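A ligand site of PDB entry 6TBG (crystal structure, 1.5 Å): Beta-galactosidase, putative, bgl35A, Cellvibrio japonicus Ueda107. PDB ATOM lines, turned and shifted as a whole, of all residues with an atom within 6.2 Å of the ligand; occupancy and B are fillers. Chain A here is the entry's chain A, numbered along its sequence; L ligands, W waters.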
ATOM      1  N   GLN A  39      18.186 -21.905  -6.025  1.00  0.00           N
ATOM      2  CA  GLN A  39      18.120 -20.986  -4.870  1.00  0.00           C
ATOM      3  C   GLN A  39      17.530 -21.766  -3.689  1.00  0.00           C
ATOM      4  O   GLN A  39      16.573 -22.511  -3.850  1.00  0.00           O
ATOM      5  CB  GLN A  39      17.337 -19.711  -5.153  1.00  0.00           C
ATOM      6  CG  GLN A  39      17.263 -18.830  -3.906  1.00  0.00           C
ATOM      7  CD  GLN A  39      16.731 -17.422  -4.078  1.00  0.00           C
ATOM      8  OE1 GLN A  39      16.254 -16.833  -3.109  1.00  0.00           O
ATOM      9  NE2 GLN A  39      16.823 -16.858  -5.277  1.00  0.00           N
ATOM     10  N   ASN A  42      14.267 -19.566   2.162  1.00  0.00           N
ATOM     11  CA  ASN A  42      14.647 -18.276   2.778  1.00  0.00           C
ATOM     12  C   ASN A  42      15.336 -18.438   4.141  1.00  0.00           C
ATOM     13  O   ASN A  42      15.900 -17.443   4.626  1.00  0.00           O
ATOM     14  CB  ASN A  42      13.412 -17.408   2.998  1.00  0.00           C
ATOM     15  CG  ASN A  42      12.910 -16.689   1.769  1.00  0.00           C
ATOM     16  OD1 ASN A  42      11.793 -16.175   1.827  1.00  0.00           O
ATOM     17  ND2 ASN A  42      13.698 -16.600   0.692  1.00  0.00           N
ATOM     18  N   PHE A 105      20.000  -9.573   1.866  1.00  0.00           N
ATOM     19  CA  PHE A 105      18.668  -9.352   2.470  1.00  0.00           C
ATOM     20  C   PHE A 105      18.837  -8.267   3.526  1.00  0.00           C
ATOM     21  O   PHE A 105      19.479  -8.538   4.550  1.00  0.00           O
ATOM     22  CB  PHE A 105      18.121 -10.649   3.071  1.00  0.00           C
ATOM     23  CG  PHE A 105      17.520 -11.679   2.145  1.00  0.00           C
ATOM     24  CD1 PHE A 105      17.661 -11.613   0.763  1.00  0.00           C
ATOM     25  CD2 PHE A 105      16.849 -12.760   2.682  1.00  0.00           C
ATOM     26  CE1 PHE A 105      17.096 -12.582  -0.046  1.00  0.00           C
ATOM     27  CE2 PHE A 105      16.304 -13.741   1.873  1.00  0.00           C
ATOM     28  CZ  PHE A 105      16.444 -13.659   0.504  1.00  0.00           C
ATOM     29  N   LYS A 109      13.388  -7.014   2.012  1.00  0.00           N
ATOM     30  CA  LYS A 109      13.175  -8.410   1.597  1.00  0.00           C
ATOM     31  C   LYS A 109      11.660  -8.578   1.452  1.00  0.00           C
ATOM     32  O   LYS A 109      10.938  -8.503   2.480  1.00  0.00           O
ATOM     33  CB  LYS A 109      13.839  -9.341   2.626  1.00  0.00           C
ATOM     34  CG  LYS A 109      14.032 -10.776   2.167  1.00  0.00           C
ATOM     35  CD  LYS A 109      12.718 -11.503   1.955  1.00  0.00           C
ATOM     36  CE  LYS A 109      12.875 -12.964   1.584  1.00  0.00           C
ATOM     37  NZ  LYS A 109      11.566 -13.539   1.177  1.00  0.00           N
ATOM     38  N   ASN A 110      11.170  -8.706   0.230  1.00  0.00           N
ATOM     39  CA  ASN A 110       9.720  -8.771  -0.062  1.00  0.00           C
ATOM     40  C   ASN A 110       9.020  -7.565   0.579  1.00  0.00           C
ATOM     41  O   ASN A 110       8.028  -7.755   1.309  1.00  0.00           O
ATOM     42  CB  ASN A 110       9.105 -10.091   0.437  1.00  0.00           C
ATOM     43  CG  ASN A 110       9.617 -11.320  -0.270  1.00  0.00           C
ATOM     44  OD1 ASN A 110      10.765 -11.369  -0.736  1.00  0.00           O
ATOM     45  ND2 ASN A 110       8.797 -12.369  -0.278  1.00  0.00           N
ATOM     46  N   ASN A 179      16.071  -7.679  -1.842  1.00  0.00           N
ATOM     47  CA  ASN A 179      15.249  -8.774  -2.399  1.00  0.00           C
ATOM     48  C   ASN A 179      13.811  -8.285  -2.554  1.00  0.00           C
ATOM     49  O   ASN A 179      13.193  -7.923  -1.546  1.00  0.00           O
ATOM     50  CB  ASN A 179      15.307 -10.047  -1.559  1.00  0.00           C
ATOM     51  CG  ASN A 179      14.594 -11.188  -2.240  1.00  0.00           C
ATOM     52  OD1 ASN A 179      15.208 -11.877  -3.048  1.00  0.00           O
ATOM     53  ND2 ASN A 179      13.306 -11.345  -1.976  1.00  0.00           N
ATOM     54  N   GLU A 180      13.323  -8.232  -3.788  1.00  0.00           N
ATOM     55  CA  GLU A 180      11.928  -7.817  -4.115  1.00  0.00           C
ATOM     56  C   GLU A 180      11.589  -6.539  -3.342  1.00  0.00           C
ATOM     57  O   GLU A 180      10.750  -6.542  -2.434  1.00  0.00           O
ATOM     58  CB  GLU A 180      10.976  -8.986  -3.884  1.00  0.00           C
ATOM     59  CG  GLU A 180      11.140 -10.113  -4.895  1.00  0.00           C
ATOM     60  CD  GLU A 180      10.002 -11.117  -4.952  1.00  0.00           C
ATOM     61  OE1 GLU A 180       9.220 -11.197  -3.979  1.00  0.00           O
ATOM     62  OE2 GLU A 180       9.889 -11.815  -5.980  1.00  0.00           O
ATOM     63  N   TYR A 184       3.913  -3.081  -0.381  1.00  0.00           N
ATOM     64  CA  TYR A 184       2.535  -3.614  -0.471  1.00  0.00           C
ATOM     65  C   TYR A 184       1.652  -2.721   0.399  1.00  0.00           C
ATOM     66  O   TYR A 184       2.068  -2.382   1.536  1.00  0.00           O
ATOM     67  CB  TYR A 184       2.475  -5.068  -0.001  1.00  0.00           C
ATOM     68  CG  TYR A 184       3.138  -6.070  -0.901  1.00  0.00           C
ATOM     69  CD1 TYR A 184       2.625  -6.353  -2.158  1.00  0.00           C
ATOM     70  CD2 TYR A 184       4.264  -6.782  -0.493  1.00  0.00           C
ATOM     71  CE1 TYR A 184       3.216  -7.285  -2.991  1.00  0.00           C
ATOM     72  CE2 TYR A 184       4.868  -7.717  -1.307  1.00  0.00           C
ATOM     73  CZ  TYR A 184       4.328  -7.986  -2.567  1.00  0.00           C
ATOM     74  OH  TYR A 184       4.913  -8.909  -3.381  1.00  0.00           O
ATOM     75  N   ASN A 256      16.028  -8.031  -8.134  1.00  0.00           N
ATOM     76  CA  ASN A 256      15.021  -9.026  -8.531  1.00  0.00           C
ATOM     77  C   ASN A 256      13.619  -8.494  -8.238  1.00  0.00           C
ATOM     78  O   ASN A 256      13.370  -7.955  -7.145  1.00  0.00           O
ATOM     79  CB  ASN A 256      15.261 -10.370  -7.856  1.00  0.00           C
ATOM     80  CG  ASN A 256      15.098 -10.318  -6.367  1.00  0.00           C
ATOM     81  OD1 ASN A 256      15.528  -9.344  -5.729  1.00  0.00           O
ATOM     82  ND2 ASN A 256      14.580 -11.398  -5.803  1.00  0.00           N
ATOM     83  N   ALA A 258       9.543  -8.549  -7.770  1.00  0.00           N
ATOM     84  CA  ALA A 258       8.200  -9.093  -7.474  1.00  0.00           C
ATOM     85  C   ALA A 258       7.300  -8.619  -8.619  1.00  0.00           C
ATOM     86  O   ALA A 258       6.838  -7.446  -8.585  1.00  0.00           O
ATOM     87  CB  ALA A 258       7.738  -8.633  -6.135  1.00  0.00           C
ATOM     88  N   LEU A 259       7.168  -9.451  -9.646  1.00  0.00           N
ATOM     89  CA  LEU A 259       6.511  -9.060 -10.920  1.00  0.00           C
ATOM     90  C   LEU A 259       5.061  -8.656 -10.666  1.00  0.00           C
ATOM     91  O   LEU A 259       4.370  -9.338  -9.873  1.00  0.00           O
ATOM     92  CB  LEU A 259       6.546 -10.207 -11.918  1.00  0.00           C
ATOM     93  CG  LEU A 259       7.945 -10.677 -12.316  1.00  0.00           C
ATOM     94  CD1 LEU A 259       7.842 -11.946 -13.151  1.00  0.00           C
ATOM     95  CD2 LEU A 259       8.704  -9.573 -13.059  1.00  0.00           C
ATOM     96  N   ASP A 297      11.316 -12.402 -11.208  1.00  0.00           N
ATOM     97  CA  ASP A 297      11.024 -13.568 -10.322  1.00  0.00           C
ATOM     98  C   ASP A 297       9.704 -14.186 -10.788  1.00  0.00           C
ATOM     99  O   ASP A 297       8.646 -13.591 -10.539  1.00  0.00           O
ATOM    100  CB  ASP A 297      10.944 -13.136  -8.856  1.00  0.00           C
ATOM    101  CG  ASP A 297      12.220 -12.590  -8.247  1.00  0.00           C
ATOM    102  OD1 ASP A 297      13.297 -12.822  -8.813  1.00  0.00           O
ATOM    103  OD2 ASP A 297      12.119 -11.920  -7.188  1.00  0.00           O
ATOM    104  N   ILE A 298       9.758 -15.320 -11.489  1.00  0.00           N
ATOM    105  CA  ILE A 298       8.595 -15.804 -12.285  1.00  0.00           C
ATOM    106  C   ILE A 298       7.853 -16.890 -11.516  1.00  0.00           C
ATOM    107  O   ILE A 298       8.394 -18.010 -11.373  1.00  0.00           O
ATOM    108  CB  ILE A 298       9.041 -16.291 -13.656  1.00  0.00           C
ATOM    109  CG1 ILE A 298       9.775 -15.158 -14.373  1.00  0.00           C
ATOM    110  CG2 ILE A 298       7.848 -16.804 -14.450  1.00  0.00           C
ATOM    111  CD1 ILE A 298      10.369 -15.541 -15.730  1.00  0.00           C
ATOM    112  N   TYR A 299       6.613 -16.596 -11.129  1.00  0.00           N
ATOM    113  CA  TYR A 299       5.718 -17.606 -10.494  1.00  0.00           C
ATOM    114  C   TYR A 299       4.408 -17.742 -11.263  1.00  0.00           C
ATOM    115  O   TYR A 299       3.547 -18.535 -10.865  1.00  0.00           O
ATOM    116  CB  TYR A 299       5.544 -17.275  -9.009  1.00  0.00           C
ATOM    117  CG  TYR A 299       6.838 -17.361  -8.243  1.00  0.00           C
ATOM    118  CD1 TYR A 299       7.389 -18.594  -7.920  1.00  0.00           C
ATOM    119  CD2 TYR A 299       7.580 -16.233  -7.932  1.00  0.00           C
ATOM    120  CE1 TYR A 299       8.605 -18.686  -7.245  1.00  0.00           C
ATOM    121  CE2 TYR A 299       8.791 -16.317  -7.267  1.00  0.00           C
ATOM    122  CZ  TYR A 299       9.307 -17.547  -6.904  1.00  0.00           C
ATOM    123  OH  TYR A 299      10.506 -17.650  -6.248  1.00  0.00           O
ATOM    124  N   PHE A 300       4.277 -17.080 -12.411  1.00  0.00           N
ATOM    125  CA  PHE A 300       3.129 -17.310 -13.334  1.00  0.00           C
ATOM    126  C   PHE A 300       3.383 -18.666 -14.007  1.00  0.00           C
ATOM    127  O   PHE A 300       4.513 -18.862 -14.455  1.00  0.00           O
ATOM    128  CB  PHE A 300       3.041 -16.205 -14.382  1.00  0.00           C
ATOM    129  CG  PHE A 300       3.033 -14.810 -13.829  1.00  0.00           C
ATOM    130  CD1 PHE A 300       2.017 -14.394 -12.979  1.00  0.00           C
ATOM    131  CD2 PHE A 300       4.024 -13.900 -14.153  1.00  0.00           C
ATOM    132  CE1 PHE A 300       2.014 -13.111 -12.450  1.00  0.00           C
ATOM    133  CE2 PHE A 300       4.015 -12.608 -13.634  1.00  0.00           C
ATOM    134  CZ  PHE A 300       3.011 -12.224 -12.777  1.00  0.00           C
ATOM    135  N   ARG A 301       2.422 -19.587 -14.023  1.00  0.00           N
ATOM    136  CA  ARG A 301       2.643 -20.952 -14.577  1.00  0.00           C
ATOM    137  C   ARG A 301       2.350 -20.984 -16.082  1.00  0.00           C
ATOM    138  O   ARG A 301       3.030 -21.780 -16.805  1.00  0.00           O
ATOM    139  CB  ARG A 301       1.760 -21.984 -13.868  1.00  0.00           C
ATOM    140  CG  ARG A 301       2.211 -22.233 -12.438  1.00  0.00           C
ATOM    141  CD  ARG A 301       1.092 -22.347 -11.421  1.00  0.00           C
ATOM    142  NE  ARG A 301       1.706 -22.749 -10.152  1.00  0.00           N
ATOM    143  CZ  ARG A 301       2.116 -23.979  -9.890  1.00  0.00           C
ATOM    144  NH1 ARG A 301       1.993 -24.933 -10.804  1.00  0.00           N
ATOM    145  NH2 ARG A 301       2.686 -24.265  -8.732  1.00  0.00           N
ATOM    146  N   GLU A 324      14.669 -15.998 -10.110  1.00  0.00           N
ATOM    147  CA  GLU A 324      13.818 -16.995  -9.438  1.00  0.00           C
ATOM    148  C   GLU A 324      12.778 -17.501 -10.416  1.00  0.00           C
ATOM    149  O   GLU A 324      12.224 -16.690 -11.217  1.00  0.00           O
ATOM    150  CB  GLU A 324      13.027 -16.412  -8.257  1.00  0.00           C
ATOM    151  CG  GLU A 324      13.865 -15.825  -7.145  1.00  0.00           C
ATOM    152  CD  GLU A 324      13.054 -15.095  -6.091  1.00  0.00           C
ATOM    153  OE1 GLU A 324      11.852 -15.379  -5.965  1.00  0.00           O
ATOM    154  OE2 GLU A 324      13.616 -14.231  -5.406  1.00  0.00           O
ATOM    155  N   PHE A 349      13.542 -21.664  -7.487  1.00  0.00           N
ATOM    156  CA  PHE A 349      13.469 -21.272  -6.066  1.00  0.00           C
ATOM    157  C   PHE A 349      13.029 -22.447  -5.197  1.00  0.00           C
ATOM    158  O   PHE A 349      12.064 -23.145  -5.523  1.00  0.00           O
ATOM    159  CB  PHE A 349      12.485 -20.117  -5.915  1.00  0.00           C
ATOM    160  CG  PHE A 349      12.434 -19.665  -4.487  1.00  0.00           C
ATOM    161  CD1 PHE A 349      13.332 -18.735  -4.006  1.00  0.00           C
ATOM    162  CD2 PHE A 349      11.524 -20.241  -3.620  1.00  0.00           C
ATOM    163  CE1 PHE A 349      13.312 -18.351  -2.679  1.00  0.00           C
ATOM    164  CE2 PHE A 349      11.528 -19.877  -2.283  1.00  0.00           C
ATOM    165  CZ  PHE A 349      12.406 -18.937  -1.832  1.00  0.00           C
ATOM    166  N   TYR A 356      10.127 -27.274   3.627  1.00  0.00           N
ATOM    167  CA  TYR A 356       9.286 -26.134   3.235  1.00  0.00           C
ATOM    168  C   TYR A 356       8.956 -26.243   1.757  1.00  0.00           C
ATOM    169  O   TYR A 356       9.823 -26.542   0.943  1.00  0.00           O
ATOM    170  CB  TYR A 356       9.955 -24.793   3.521  1.00  0.00           C
ATOM    171  CG  TYR A 356       9.006 -23.651   3.318  1.00  0.00           C
ATOM    172  CD1 TYR A 356       8.135 -23.257   4.330  1.00  0.00           C
ATOM    173  CD2 TYR A 356       8.963 -22.975   2.115  1.00  0.00           C
ATOM    174  CE1 TYR A 356       7.223 -22.232   4.129  1.00  0.00           C
ATOM    175  CE2 TYR A 356       8.064 -21.946   1.911  1.00  0.00           C
ATOM    176  CZ  TYR A 356       7.190 -21.574   2.917  1.00  0.00           C
ATOM    177  OH  TYR A 356       6.305 -20.549   2.703  1.00  0.00           O
ATOM    178  N   ASN A 358       6.839 -23.566  -1.111  1.00  0.00           N
ATOM    179  CA  ASN A 358       6.093 -22.291  -1.315  1.00  0.00           C
ATOM    180  C   ASN A 358       4.860 -22.514  -2.207  1.00  0.00           C
ATOM    181  O   ASN A 358       4.265 -21.506  -2.610  1.00  0.00           O
ATOM    182  CB  ASN A 358       6.977 -21.173  -1.847  1.00  0.00           C
ATOM    183  CG  ASN A 358       7.484 -21.391  -3.251  1.00  0.00           C
ATOM    184  OD1 ASN A 358       7.286 -22.447  -3.834  1.00  0.00           O
ATOM    185  ND2 ASN A 358       8.124 -20.376  -3.775  1.00  0.00           N
ATOM    186  N   LEU A 361       2.831 -21.315  -5.138  1.00  0.00           N
ATOM    187  CA  LEU A 361       3.834 -20.786  -6.112  1.00  0.00           C
ATOM    188  C   LEU A 361       4.634 -21.956  -6.709  1.00  0.00           C
ATOM    189  O   LEU A 361       4.758 -22.019  -7.940  1.00  0.00           O
ATOM    190  CB  LEU A 361       4.786 -19.819  -5.423  1.00  0.00           C
ATOM    191  CG  LEU A 361       4.186 -18.530  -4.856  1.00  0.00           C
ATOM    192  CD1 LEU A 361       5.283 -17.543  -4.504  1.00  0.00           C
ATOM    193  CD2 LEU A 361       3.191 -17.903  -5.817  1.00  0.00           C
HETATM  194  C1  LIG L   1       9.824 -14.668  -3.675  1.00  0.00           C
HETATM  195  C2  LIG L   1       9.776 -16.060  -3.013  1.00  0.00           C
HETATM  196  O1  LIG L   1       0.721 -16.489  -8.713  1.00  0.00           O
HETATM  197  C3  LIG L   1      10.600 -15.851  -1.767  1.00  0.00           C
HETATM  198  C4  LIG L   1       8.398 -16.686  -2.824  1.00  0.00           C
HETATM  199  C5  LIG L   1       7.555 -14.118  -4.668  1.00  0.00           C
HETATM  200  C6  LIG L   1      11.771 -15.049  -2.304  1.00  0.00           C
HETATM  201  C7  LIG L   1      10.981 -13.923  -2.970  1.00  0.00           C
HETATM  202  N1  LIG L   1       8.559 -13.891  -3.582  1.00  0.00           N
HETATM  203  O2  LIG L   1       8.579 -17.997  -2.238  1.00  0.00           O
HETATM  204  O3  LIG L   1       9.881 -15.066  -0.816  1.00  0.00           O
HETATM  205  O4  LIG L   1      12.662 -14.538  -1.331  1.00  0.00           O
HETATM  206  O5  LIG L   1      11.830 -13.106  -3.816  1.00  0.00           O
HETATM  207  C8  LIG L   1       6.221 -13.401  -4.448  1.00  0.00           C
HETATM  208  C9  LIG L   1       5.324 -13.584  -5.654  1.00  0.00           C
HETATM  209  C10 LIG L   1       3.865 -13.280  -5.407  1.00  0.00           C
HETATM  210  C11 LIG L   1       3.036 -13.132  -6.687  1.00  0.00           C
HETATM  211  C12 LIG L   1       2.635 -14.456  -7.358  1.00  0.00           C
HETATM  212  N2  LIG L   1       1.483 -14.168  -8.244  1.00  0.00           N
HETATM  213  S1  LIG L   1       1.278 -15.312  -9.357  1.00  0.00           S
HETATM  214  O6  LIG L   1       2.506 -15.641 -10.013  1.00  0.00           O
HETATM  215  O   HOH W   1       6.548 -13.992  -1.308  1.00  0.00           O
HETATM  216  O   HOH W   2       5.016 -12.097  -9.044  1.00  0.00           O
HETATM  217  O   HOH W   3       5.239 -14.172 -10.805  1.00  0.00           O
HETATM  218  O   HOH W   4      15.097 -14.542  -2.408  1.00  0.00           O
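The side-chain carboxylate of Asp 297 sits at hydrogen-bond distance from the side-chain amide nitrogen of Asn 256 (2.9 Å). NZ of Lys 109 sits at hydrogen-bond distance from OD1 of Asn 42 (2.7 Å). The side-chain carboxylate (OE2) of Glu 180 lies close to the side-chain carboxylate (OD2) of Asp 297 (2.5 Å). The side-chain carboxylate of Glu 324 sits at hydrogen-bond distance from the side-chain hydroxyl of Tyr 299 (2.7 Å). The backbone carbonyl oxygen (O) of Glu 324 lies within hydrogen-bond range of the backbone NH (N) of Ile 298 (2.8 Å). O of Leu 361 is in hydrogen-bond range of NH2 of Arg 301, 3.2 Å away. The backbone NH (N) of Glu 180 is in hydrogen-bond range of the side-chain amide oxygen (OD1) of Asn 256 (3.1 Å). The backbone carbonyl oxygen (O) of Glu 180 sits close to the backbone NH (N) of Asn 110 (3.5 Å).
Water W1 bridges the side-chain amide nitrogen of Asn 110 (3.0 Å) and a nitrogen (N1) of the ligand (3.0 Å). Water W3 lies within hydrogen-bond range of the backbone NH (N) of Tyr 299 (2.8 Å), an oxygen (O6) of the ligand (3.2 Å), the backbone NH (N) of Phe 300 (3.5 Å) and the backbone carbonyl oxygen (O) of Asp 297 (3.5 Å).
OE1 of Glu 180 is in salt-bridge range of N1 of the ligand (2.8 Å). ND2 of Asn 358 lies within hydrogen-bond range of O2 of the ligand, 2.9 Å away. The backbone NH (N) of Phe 300 sits close to an oxygen (O6) of the ligand (3.3 Å). O4 of the ligand is in hydrogen-bond range of NZ of Lys 109 (2.9 Å). The side-chain amide nitrogen (ND2) of Asn 179 sits at hydrogen-bond distance from an oxygen (O5) of the ligand, 2.9 Å away. An oxygen (O5) of the ligand is in hydrogen-bond range of the side-chain carboxylate of Glu 324 (2.6 Å). The side-chain amide nitrogen (ND2) of Asn 42 is in hydrogen-bond range of an oxygen (O4) of the ligand (3.1 Å). ND2 of Asn 110 is in hydrogen-bond range of O3 of the ligand, 3.0 Å away.
The backbone carbonyl oxygen (O) of Tyr 299 lies close to an oxygen (O6) of the ligand, 3.2 Å away. Asn 256 touches the ligand. Asp 297 touches the ligand. CE2 of Phe 349 touches O2 of the ligand, at 3.5 Å. Leu 361 touches the ligand. Hydrophobic or aromatic side chains within 4 Å of the ligand: Tyr 299, Phe 300, Phe 349 and Leu 361. Of the 21 residues printed, 13 come within 4 Å of the ligand. The nearest printed residue that does not touch the ligand is Phe 105 (4.3 Å).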
